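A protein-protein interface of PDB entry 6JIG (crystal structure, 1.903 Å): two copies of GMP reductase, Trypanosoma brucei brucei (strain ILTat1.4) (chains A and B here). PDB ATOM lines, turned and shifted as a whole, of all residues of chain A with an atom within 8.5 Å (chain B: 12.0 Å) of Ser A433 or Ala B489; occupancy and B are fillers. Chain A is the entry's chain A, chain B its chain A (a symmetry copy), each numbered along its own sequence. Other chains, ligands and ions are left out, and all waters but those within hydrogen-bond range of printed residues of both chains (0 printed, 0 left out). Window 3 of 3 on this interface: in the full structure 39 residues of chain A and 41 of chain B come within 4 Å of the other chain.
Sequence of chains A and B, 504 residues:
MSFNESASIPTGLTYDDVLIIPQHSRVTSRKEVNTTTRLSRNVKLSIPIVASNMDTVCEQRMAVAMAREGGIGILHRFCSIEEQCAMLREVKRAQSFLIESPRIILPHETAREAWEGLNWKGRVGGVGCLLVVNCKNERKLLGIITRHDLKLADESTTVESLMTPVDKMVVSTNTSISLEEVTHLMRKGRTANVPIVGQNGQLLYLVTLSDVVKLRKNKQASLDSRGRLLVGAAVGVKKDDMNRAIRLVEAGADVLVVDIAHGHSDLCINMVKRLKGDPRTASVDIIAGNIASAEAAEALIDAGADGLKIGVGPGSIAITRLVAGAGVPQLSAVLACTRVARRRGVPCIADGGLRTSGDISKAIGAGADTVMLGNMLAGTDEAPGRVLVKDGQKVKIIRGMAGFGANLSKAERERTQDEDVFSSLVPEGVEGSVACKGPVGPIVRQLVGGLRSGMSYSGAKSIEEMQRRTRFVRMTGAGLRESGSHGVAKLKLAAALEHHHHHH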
ATOM      1  N   SER A 316       6.377  16.870 -17.907  1.00  0.00           N
ATOM      2  CA  SER A 316       6.752  18.285 -17.907  1.00  0.00           C
ATOM      3  C   SER A 316       6.192  19.032 -19.115  1.00  0.00           C
ATOM      4  O   SER A 316       5.707  20.162 -18.985  1.00  0.00           O
ATOM      5  CB  SER A 316       8.276  18.416 -17.879  1.00  0.00           C
ATOM      6  OG  SER A 316       8.852  17.885 -19.061  1.00  0.00           O
ATOM      7  N   ILE A 317       6.266  18.425 -20.299  1.00  0.00           N
ATOM      8  CA  ILE A 317       5.822  19.074 -21.529  1.00  0.00           C
ATOM      9  C   ILE A 317       4.434  18.590 -21.967  1.00  0.00           C
ATOM     10  O   ILE A 317       3.980  18.924 -23.062  1.00  0.00           O
ATOM     11  CB  ILE A 317       6.868  18.908 -22.653  1.00  0.00           C
ATOM     12  CG1 ILE A 317       7.186  17.438 -22.943  1.00  0.00           C
ATOM     13  CG2 ILE A 317       8.192  19.535 -22.239  1.00  0.00           C
ATOM     14  CD1 ILE A 317       6.026  16.595 -23.316  1.00  0.00           C
ATOM     15  N   ASN A 375      12.433  15.490 -18.688  1.00  0.00           N
ATOM     16  CA  ASN A 375      12.954  16.825 -18.399  1.00  0.00           C
ATOM     17  C   ASN A 375      14.265  16.795 -17.617  1.00  0.00           C
ATOM     18  O   ASN A 375      15.187  17.565 -17.910  1.00  0.00           O
ATOM     19  CB  ASN A 375      11.892  17.625 -17.632  1.00  0.00           C
ATOM     20  CG  ASN A 375      12.275  19.083 -17.450  1.00  0.00           C
ATOM     21  OD1 ASN A 375      12.919  19.685 -18.314  1.00  0.00           O
ATOM     22  ND2 ASN A 375      11.862  19.664 -16.330  1.00  0.00           N
ATOM     23  N   ALA A 378      16.903  16.052 -20.187  1.00  0.00           N
ATOM     24  CA  ALA A 378      16.999  16.913 -21.356  1.00  0.00           C
ATOM     25  C   ALA A 378      18.053  17.985 -21.108  1.00  0.00           C
ATOM     26  O   ALA A 378      18.339  18.352 -19.964  1.00  0.00           O
ATOM     27  CB  ALA A 378      15.641  17.544 -21.667  1.00  0.00           C
ATOM     28  N   GLY A 379      18.660  18.465 -22.189  1.00  0.00           N
ATOM     29  CA  GLY A 379      19.697  19.463 -22.072  1.00  0.00           C
ATOM     30  C   GLY A 379      21.027  18.954 -21.570  1.00  0.00           C
ATOM     31  O   GLY A 379      21.953  19.757 -21.388  1.00  0.00           O
ATOM     32  N   LEU A 388      21.443  26.046 -27.798  1.00  0.00           N
ATOM     33  CA  LEU A 388      20.954  27.334 -28.261  1.00  0.00           C
ATOM     34  C   LEU A 388      21.109  28.363 -27.148  1.00  0.00           C
ATOM     35  O   LEU A 388      21.183  28.021 -25.964  1.00  0.00           O
ATOM     36  CB  LEU A 388      19.488  27.251 -28.714  1.00  0.00           C
ATOM     37  N   VAL A 389      21.174  29.630 -27.546  1.00  0.00           N
ATOM     38  CA  VAL A 389      21.270  30.752 -26.619  1.00  0.00           C
ATOM     39  C   VAL A 389      19.866  31.333 -26.489  1.00  0.00           C
ATOM     40  O   VAL A 389      19.372  32.009 -27.396  1.00  0.00           O
ATOM     41  CB  VAL A 389      22.282  31.799 -27.088  1.00  0.00           C
ATOM     42  N   LYS A 390      19.214  31.054 -25.363  1.00  0.00           N
ATOM     43  CA  LYS A 390      17.862  31.539 -25.089  1.00  0.00           C
ATOM     44  C   LYS A 390      17.992  32.766 -24.195  1.00  0.00           C
ATOM     45  O   LYS A 390      17.948  32.670 -22.967  1.00  0.00           O
ATOM     46  CB  LYS A 390      17.005  30.454 -24.445  1.00  0.00           C
ATOM     47  N   ASP A 391      18.169  33.926 -24.830  1.00  0.00           N
ATOM     48  CA  ASP A 391      18.248  35.216 -24.143  1.00  0.00           C
ATOM     49  C   ASP A 391      19.341  35.219 -23.074  1.00  0.00           C
ATOM     50  O   ASP A 391      19.116  35.585 -21.918  1.00  0.00           O
ATOM     51  CB  ASP A 391      16.892  35.599 -23.545  1.00  0.00           C
ATOM     52  N   GLN A 393      21.783  32.594 -21.828  1.00  0.00           N
ATOM     53  CA  GLN A 393      22.441  31.371 -21.390  1.00  0.00           C
ATOM     54  C   GLN A 393      22.288  30.263 -22.430  1.00  0.00           C
ATOM     55  O   GLN A 393      21.514  30.367 -23.385  1.00  0.00           O
ATOM     56  CB  GLN A 393      21.882  30.919 -20.035  1.00  0.00           C
ATOM     57  N   LYS A 394      23.052  29.188 -22.230  1.00  0.00           N
ATOM     58  CA  LYS A 394      23.022  28.045 -23.135  1.00  0.00           C
ATOM     59  C   LYS A 394      21.873  27.114 -22.762  1.00  0.00           C
ATOM     60  O   LYS A 394      21.726  26.729 -21.595  1.00  0.00           O
ATOM     61  CB  LYS A 394      24.354  27.295 -23.096  1.00  0.00           C
ATOM     62  N   VAL A 395      21.060  26.751 -23.759  1.00  0.00           N
ATOM     63  CA  VAL A 395      19.843  25.975 -23.555  1.00  0.00           C
ATOM     64  C   VAL A 395      19.751  24.889 -24.623  1.00  0.00           C
ATOM     65  O   VAL A 395      20.471  24.901 -25.623  1.00  0.00           O
ATOM     66  CB  VAL A 395      18.577  26.862 -23.589  1.00  0.00           C
ATOM     67  N   LYS A 396      18.845  23.941 -24.390  1.00  0.00           N
ATOM     68  CA  LYS A 396      18.470  22.935 -25.376  1.00  0.00           C
ATOM     69  C   LYS A 396      16.952  22.814 -25.400  1.00  0.00           C
ATOM     70  O   LYS A 396      16.271  23.103 -24.413  1.00  0.00           O
ATOM     71  CB  LYS A 396      19.102  21.561 -25.076  1.00  0.00           C
ATOM     72  CG  LYS A 396      20.521  21.378 -25.604  1.00  0.00           C
ATOM     73  CD  LYS A 396      20.925  19.898 -25.628  1.00  0.00           C
ATOM     74  CE  LYS A 396      22.394  19.734 -25.961  1.00  0.00           C
ATOM     75  NZ  LYS A 396      22.735  18.313 -26.242  1.00  0.00           N
ATOM     76  N   ILE A 397      16.425  22.376 -26.541  1.00  0.00           N
ATOM     77  CA  ILE A 397      14.984  22.224 -26.711  1.00  0.00           C
ATOM     78  C   ILE A 397      14.511  20.965 -25.998  1.00  0.00           C
ATOM     79  O   ILE A 397      15.174  19.919 -26.033  1.00  0.00           O
ATOM     80  CB  ILE A 397      14.619  22.183 -28.208  1.00  0.00           C
ATOM     81  CG1 ILE A 397      14.947  23.517 -28.881  1.00  0.00           C
ATOM     82  CG2 ILE A 397      13.142  21.838 -28.399  1.00  0.00           C
ATOM     83  CD1 ILE A 397      14.279  24.707 -28.227  1.00  0.00           C
ATOM     84  N   ILE A 398      13.364  21.069 -25.326  1.00  0.00           N
ATOM     85  CA  ILE A 398      12.580  19.915 -24.901  1.00  0.00           C
ATOM     86  C   ILE A 398      11.166  20.110 -25.436  1.00  0.00           C
ATOM     87  O   ILE A 398      10.632  21.226 -25.408  1.00  0.00           O
ATOM     88  CB  ILE A 398      12.589  19.732 -23.365  1.00  0.00           C
ATOM     89  CG1 ILE A 398      11.987  18.376 -22.978  1.00  0.00           C
ATOM     90  CG2 ILE A 398      11.874  20.899 -22.650  1.00  0.00           C
ATOM     91  CD1 ILE A 398      11.913  18.157 -21.480  1.00  0.00           C
ATOM     92  N   ARG A 399      10.574  19.042 -25.969  1.00  0.00           N
ATOM     93  CA  ARG A 399       9.279  19.192 -26.614  1.00  0.00           C
ATOM     94  C   ARG A 399       8.455  17.922 -26.461  1.00  0.00           C
ATOM     95  O   ARG A 399       8.986  16.804 -26.451  1.00  0.00           O
ATOM     96  CB  ARG A 399       9.435  19.556 -28.098  1.00  0.00           C
ATOM     97  CG  ARG A 399       9.989  18.444 -28.967  1.00  0.00           C
ATOM     98  CD  ARG A 399      10.410  18.993 -30.309  1.00  0.00           C
ATOM     99  NE  ARG A 399      10.919  17.948 -31.189  1.00  0.00           N
ATOM    100  CZ  ARG A 399      11.525  18.192 -32.346  1.00  0.00           C
ATOM    101  NH1 ARG A 399      11.688  19.448 -32.747  1.00  0.00           N
ATOM    102  NH2 ARG A 399      11.965  17.189 -33.098  1.00  0.00           N
ATOM    103  N   VAL A 430       3.802  20.456 -25.572  1.00  0.00           N
ATOM    104  CA  VAL A 430       4.324  21.784 -25.870  1.00  0.00           C
ATOM    105  C   VAL A 430       5.821  21.688 -26.151  1.00  0.00           C
ATOM    106  O   VAL A 430       6.448  20.647 -25.959  1.00  0.00           O
ATOM    107  CB  VAL A 430       4.051  22.792 -24.732  1.00  0.00           C
ATOM    108  CG1 VAL A 430       2.557  22.938 -24.495  1.00  0.00           C
ATOM    109  CG2 VAL A 430       4.775  22.371 -23.456  1.00  0.00           C
ATOM    110  N   GLU A 431       6.384  22.802 -26.615  1.00  0.00           N
ATOM    111  CA  GLU A 431       7.820  22.956 -26.794  1.00  0.00           C
ATOM    112  C   GLU A 431       8.364  24.004 -25.828  1.00  0.00           C
ATOM    113  O   GLU A 431       7.668  24.953 -25.451  1.00  0.00           O
ATOM    114  CB  GLU A 431       8.158  23.348 -28.237  1.00  0.00           C
ATOM    115  N   GLY A 432       9.619  23.819 -25.429  1.00  0.00           N
ATOM    116  CA  GLY A 432      10.287  24.753 -24.543  1.00  0.00           C
ATOM    117  C   GLY A 432      11.780  24.510 -24.557  1.00  0.00           C
ATOM    118  O   GLY A 432      12.290  23.651 -25.281  1.00  0.00           O
ATOM    119  N   SER A 433      12.486  25.290 -23.741  1.00  0.00           N
ATOM    120  CA  SER A 433      13.928  25.165 -23.601  1.00  0.00           C
ATOM    121  C   SER A 433      14.274  24.773 -22.171  1.00  0.00           C
ATOM    122  O   SER A 433      13.540  25.086 -21.229  1.00  0.00           O
ATOM    123  CB  SER A 433      14.649  26.474 -23.971  1.00  0.00           C
ATOM    124  OG  SER A 433      14.187  27.558 -23.186  1.00  0.00           O
ATOM    125  N   VAL A 434      15.393  24.066 -22.023  1.00  0.00           N
ATOM    126  CA  VAL A 434      15.969  23.760 -20.720  1.00  0.00           C
ATOM    127  C   VAL A 434      17.427  24.200 -20.738  1.00  0.00           C
ATOM    128  O   VAL A 434      18.099  24.133 -21.772  1.00  0.00           O
ATOM    129  CB  VAL A 434      15.854  22.260 -20.359  1.00  0.00           C
ATOM    130  N   ALA A 435      17.909  24.669 -19.588  1.00  0.00           N
ATOM    131  CA  ALA A 435      19.313  25.035 -19.462  1.00  0.00           C
ATOM    132  C   ALA A 435      20.204  23.819 -19.689  1.00  0.00           C
ATOM    133  O   ALA A 435      19.877  22.708 -19.266  1.00  0.00           O
ATOM    134  CB  ALA A 435      19.584  25.631 -18.078  1.00  0.00           C
ATOM    135  N   CYS A 436      21.331  24.036 -20.371  1.00  0.00           N
ATOM    136  CA  CYS A 436      22.285  22.957 -20.621  1.00  0.00           C
ATOM    137  C   CYS A 436      22.877  22.448 -19.317  1.00  0.00           C
ATOM    138  O   CYS A 436      23.398  23.227 -18.511  1.00  0.00           O
ATOM    139  CB  CYS A 436      23.401  23.447 -21.541  1.00  0.00           C
ATOM    140  SG  CYS A 436      22.901  23.561 -23.240  1.00  0.00           S
ATOM    141  N   LYS A 437      22.824  21.130 -19.125  1.00  0.00           N
ATOM    142  CA  LYS A 437      23.112  20.544 -17.823  1.00  0.00           C
ATOM    143  C   LYS A 437      24.487  19.889 -17.719  1.00  0.00           C
ATOM    144  O   LYS A 437      24.874  19.496 -16.614  1.00  0.00           O
ATOM    145  CB  LYS A 437      22.040  19.506 -17.460  1.00  0.00           C
ATOM    146  CG  LYS A 437      20.595  20.006 -17.424  1.00  0.00           C
ATOM    147  CD  LYS A 437      19.679  18.895 -16.886  1.00  0.00           C
ATOM    148  CE  LYS A 437      18.273  19.394 -16.562  1.00  0.00           C
ATOM    149  NZ  LYS A 437      17.536  19.741 -17.791  1.00  0.00           N
ATOM    150  N   GLY B 484      -0.605  21.121 -15.948  1.00  0.00           N
ATOM    151  CA  GLY B 484      -0.127  21.977 -17.015  1.00  0.00           C
ATOM    152  C   GLY B 484       1.346  21.730 -17.312  1.00  0.00           C
ATOM    153  O   GLY B 484       1.964  20.782 -16.823  1.00  0.00           O
ATOM    154  N   SER B 485       1.913  22.611 -18.133  1.00  0.00           N
ATOM    155  CA  SER B 485       3.352  22.583 -18.378  1.00  0.00           C
ATOM    156  C   SER B 485       4.108  23.013 -17.124  1.00  0.00           C
ATOM    157  O   SER B 485       3.731  23.989 -16.467  1.00  0.00           O
ATOM    158  CB  SER B 485       3.711  23.508 -19.542  1.00  0.00           C
ATOM    159  OG  SER B 485       3.386  22.909 -20.782  1.00  0.00           O
ATOM    160  N   HIS B 486       5.181  22.288 -16.791  1.00  0.00           N
ATOM    161  CA  HIS B 486       6.000  22.627 -15.635  1.00  0.00           C
ATOM    162  C   HIS B 486       7.464  22.308 -15.916  1.00  0.00           C
ATOM    163  O   HIS B 486       7.781  21.286 -16.533  1.00  0.00           O
ATOM    164  CB  HIS B 486       5.521  21.888 -14.364  1.00  0.00           C
ATOM    165  CG  HIS B 486       5.379  20.401 -14.522  1.00  0.00           C
ATOM    166  ND1 HIS B 486       6.404  19.518 -14.244  1.00  0.00           N
ATOM    167  CD2 HIS B 486       4.320  19.638 -14.892  1.00  0.00           C
ATOM    168  CE1 HIS B 486       5.988  18.281 -14.448  1.00  0.00           C
ATOM    169  NE2 HIS B 486       4.729  18.323 -14.845  1.00  0.00           N
ATOM    170  N   GLY B 487       8.354  23.199 -15.472  1.00  0.00           N
ATOM    171  CA  GLY B 487       9.785  22.961 -15.524  1.00  0.00           C
ATOM    172  C   GLY B 487      10.468  23.283 -16.835  1.00  0.00           C
ATOM    173  O   GLY B 487      11.638  22.918 -17.008  1.00  0.00           O
ATOM    174  N   VAL B 488       9.784  23.953 -17.765  1.00  0.00           N
ATOM    175  CA  VAL B 488      10.347  24.304 -19.063  1.00  0.00           C
ATOM    176  C   VAL B 488      10.001  25.757 -19.368  1.00  0.00           C
ATOM    177  O   VAL B 488       9.174  26.378 -18.699  1.00  0.00           O
ATOM    178  CB  VAL B 488       9.844  23.376 -20.190  1.00  0.00           C
ATOM    179  N   ALA B 489      10.657  26.300 -20.390  1.00  0.00           N
ATOM    180  CA  ALA B 489      10.414  27.671 -20.826  1.00  0.00           C
ATOM    181  C   ALA B 489      10.001  27.699 -22.297  1.00  0.00           C
ATOM    182  O   ALA B 489       8.809  27.705 -22.620  1.00  0.00           O
ATOM    183  CB  ALA B 489      11.654  28.529 -20.600  1.00  0.00           C
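The backbone NH (N) of His B486 lies within hydrogen-bond range of the backbone carbonyl oxygen (O) of Ser A316 (3.1 Å).
The side-chain amide nitrogen (ND2) of Asn A375 lies within hydrogen-bond range of the backbone carbonyl oxygen (O) of Gly B487 (3.3 Å).
N of Ala B489 sits at hydrogen-bond distance from O of Ser A433, at 3.2 Å.
The backbone carbonyl oxygen (O) of Ile A317 is in hydrogen-bond range of the backbone NH (N) of Val A430 (2.9 Å).
The backbone carbonyl oxygen of Asn A375 lies within hydrogen-bond range of the side-chain amino group of Lys A437 (3.2 Å).
The backbone carbonyl oxygen (O) of Ile A398 is in hydrogen-bond range of the backbone NH (N) of Gly A432 (2.8 Å).
Among the printed residues, merely in contact across the chains: Ser A316 with Ser B485 (3.4 Å), Val A430 with Ser B485 (3.1 Å), Gly A432 with Ala B489 (3.7 Å) and Ser A433 with Val B488 (3.9 Å).
Of the printed residues of chain B, Ser A316 touches Ser B485 (3.4 Å) and His B486 (3.1 Å).
Gly A379 touches none of the printed residues of chain B.
No residue of chain B comes within 4 Å of Leu A388.
No residue of chain B comes within 4 Å of Lys A390.
No residue of chain B comes within 4 Å of Val A395.
No residue of chain B comes within 4 Å of Ile A397.
No residue of chain B comes within 4 Å of Ile A398.
Of the printed residues of chain B, Val A430 touches Ser B485.
No residue of chain B comes within 4 Å of Glu A431.
Gly A432 touches just one residue of chain B: Ala B489.
Ser A433 touches just these residues of chain B: Val B488 and Ala B489.
No residue of chain B comes within 4 Å of Val A434.
Of the printed residues of chain A, Gly B487 touches Asn A375 (3.3 Å).
Of chain A, only Ser A433 (3.9 Å) comes within 4 Å of Val B488.
Ala B489 touches two residues of chain A.
The nearest residue of chain B that does not touch Ser A433 is Gly B487 (5.1 Å).
The nearest residue of chain A that does not touch Ala B489 is Glu A431 (4.1 Å).
The nearest printed residue of chain A that does not touch His B486 is Asn A375 (4.4 Å).
Printed residues of chain B that touch a printed residue of chain A: Ser B485, His B486, Gly B487, Val B488 and Ala B489.
Of the 24 printed residues of chain A, 5 touch a printed residue of chain B.
Printed residues of chain A that touch a printed residue of chain B: Ser A316, Asn A375, Val A430, Gly A432 and Ser A433.
Hydrophobic or aromatic side chains of chain A that line the printed part of chain B: Val A430.
Among the printed residues, 7 pairs touch across the chains.
Among the printed residues, no Asp or Glu carboxylate lies within 4 Å of a Lys or Arg side-chain nitrogen of the other chain.
No position is printed for both chains.
Of the 7 pairs that touch across the chains among the printed residues, none has its exchanged pair printed and touching as well.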
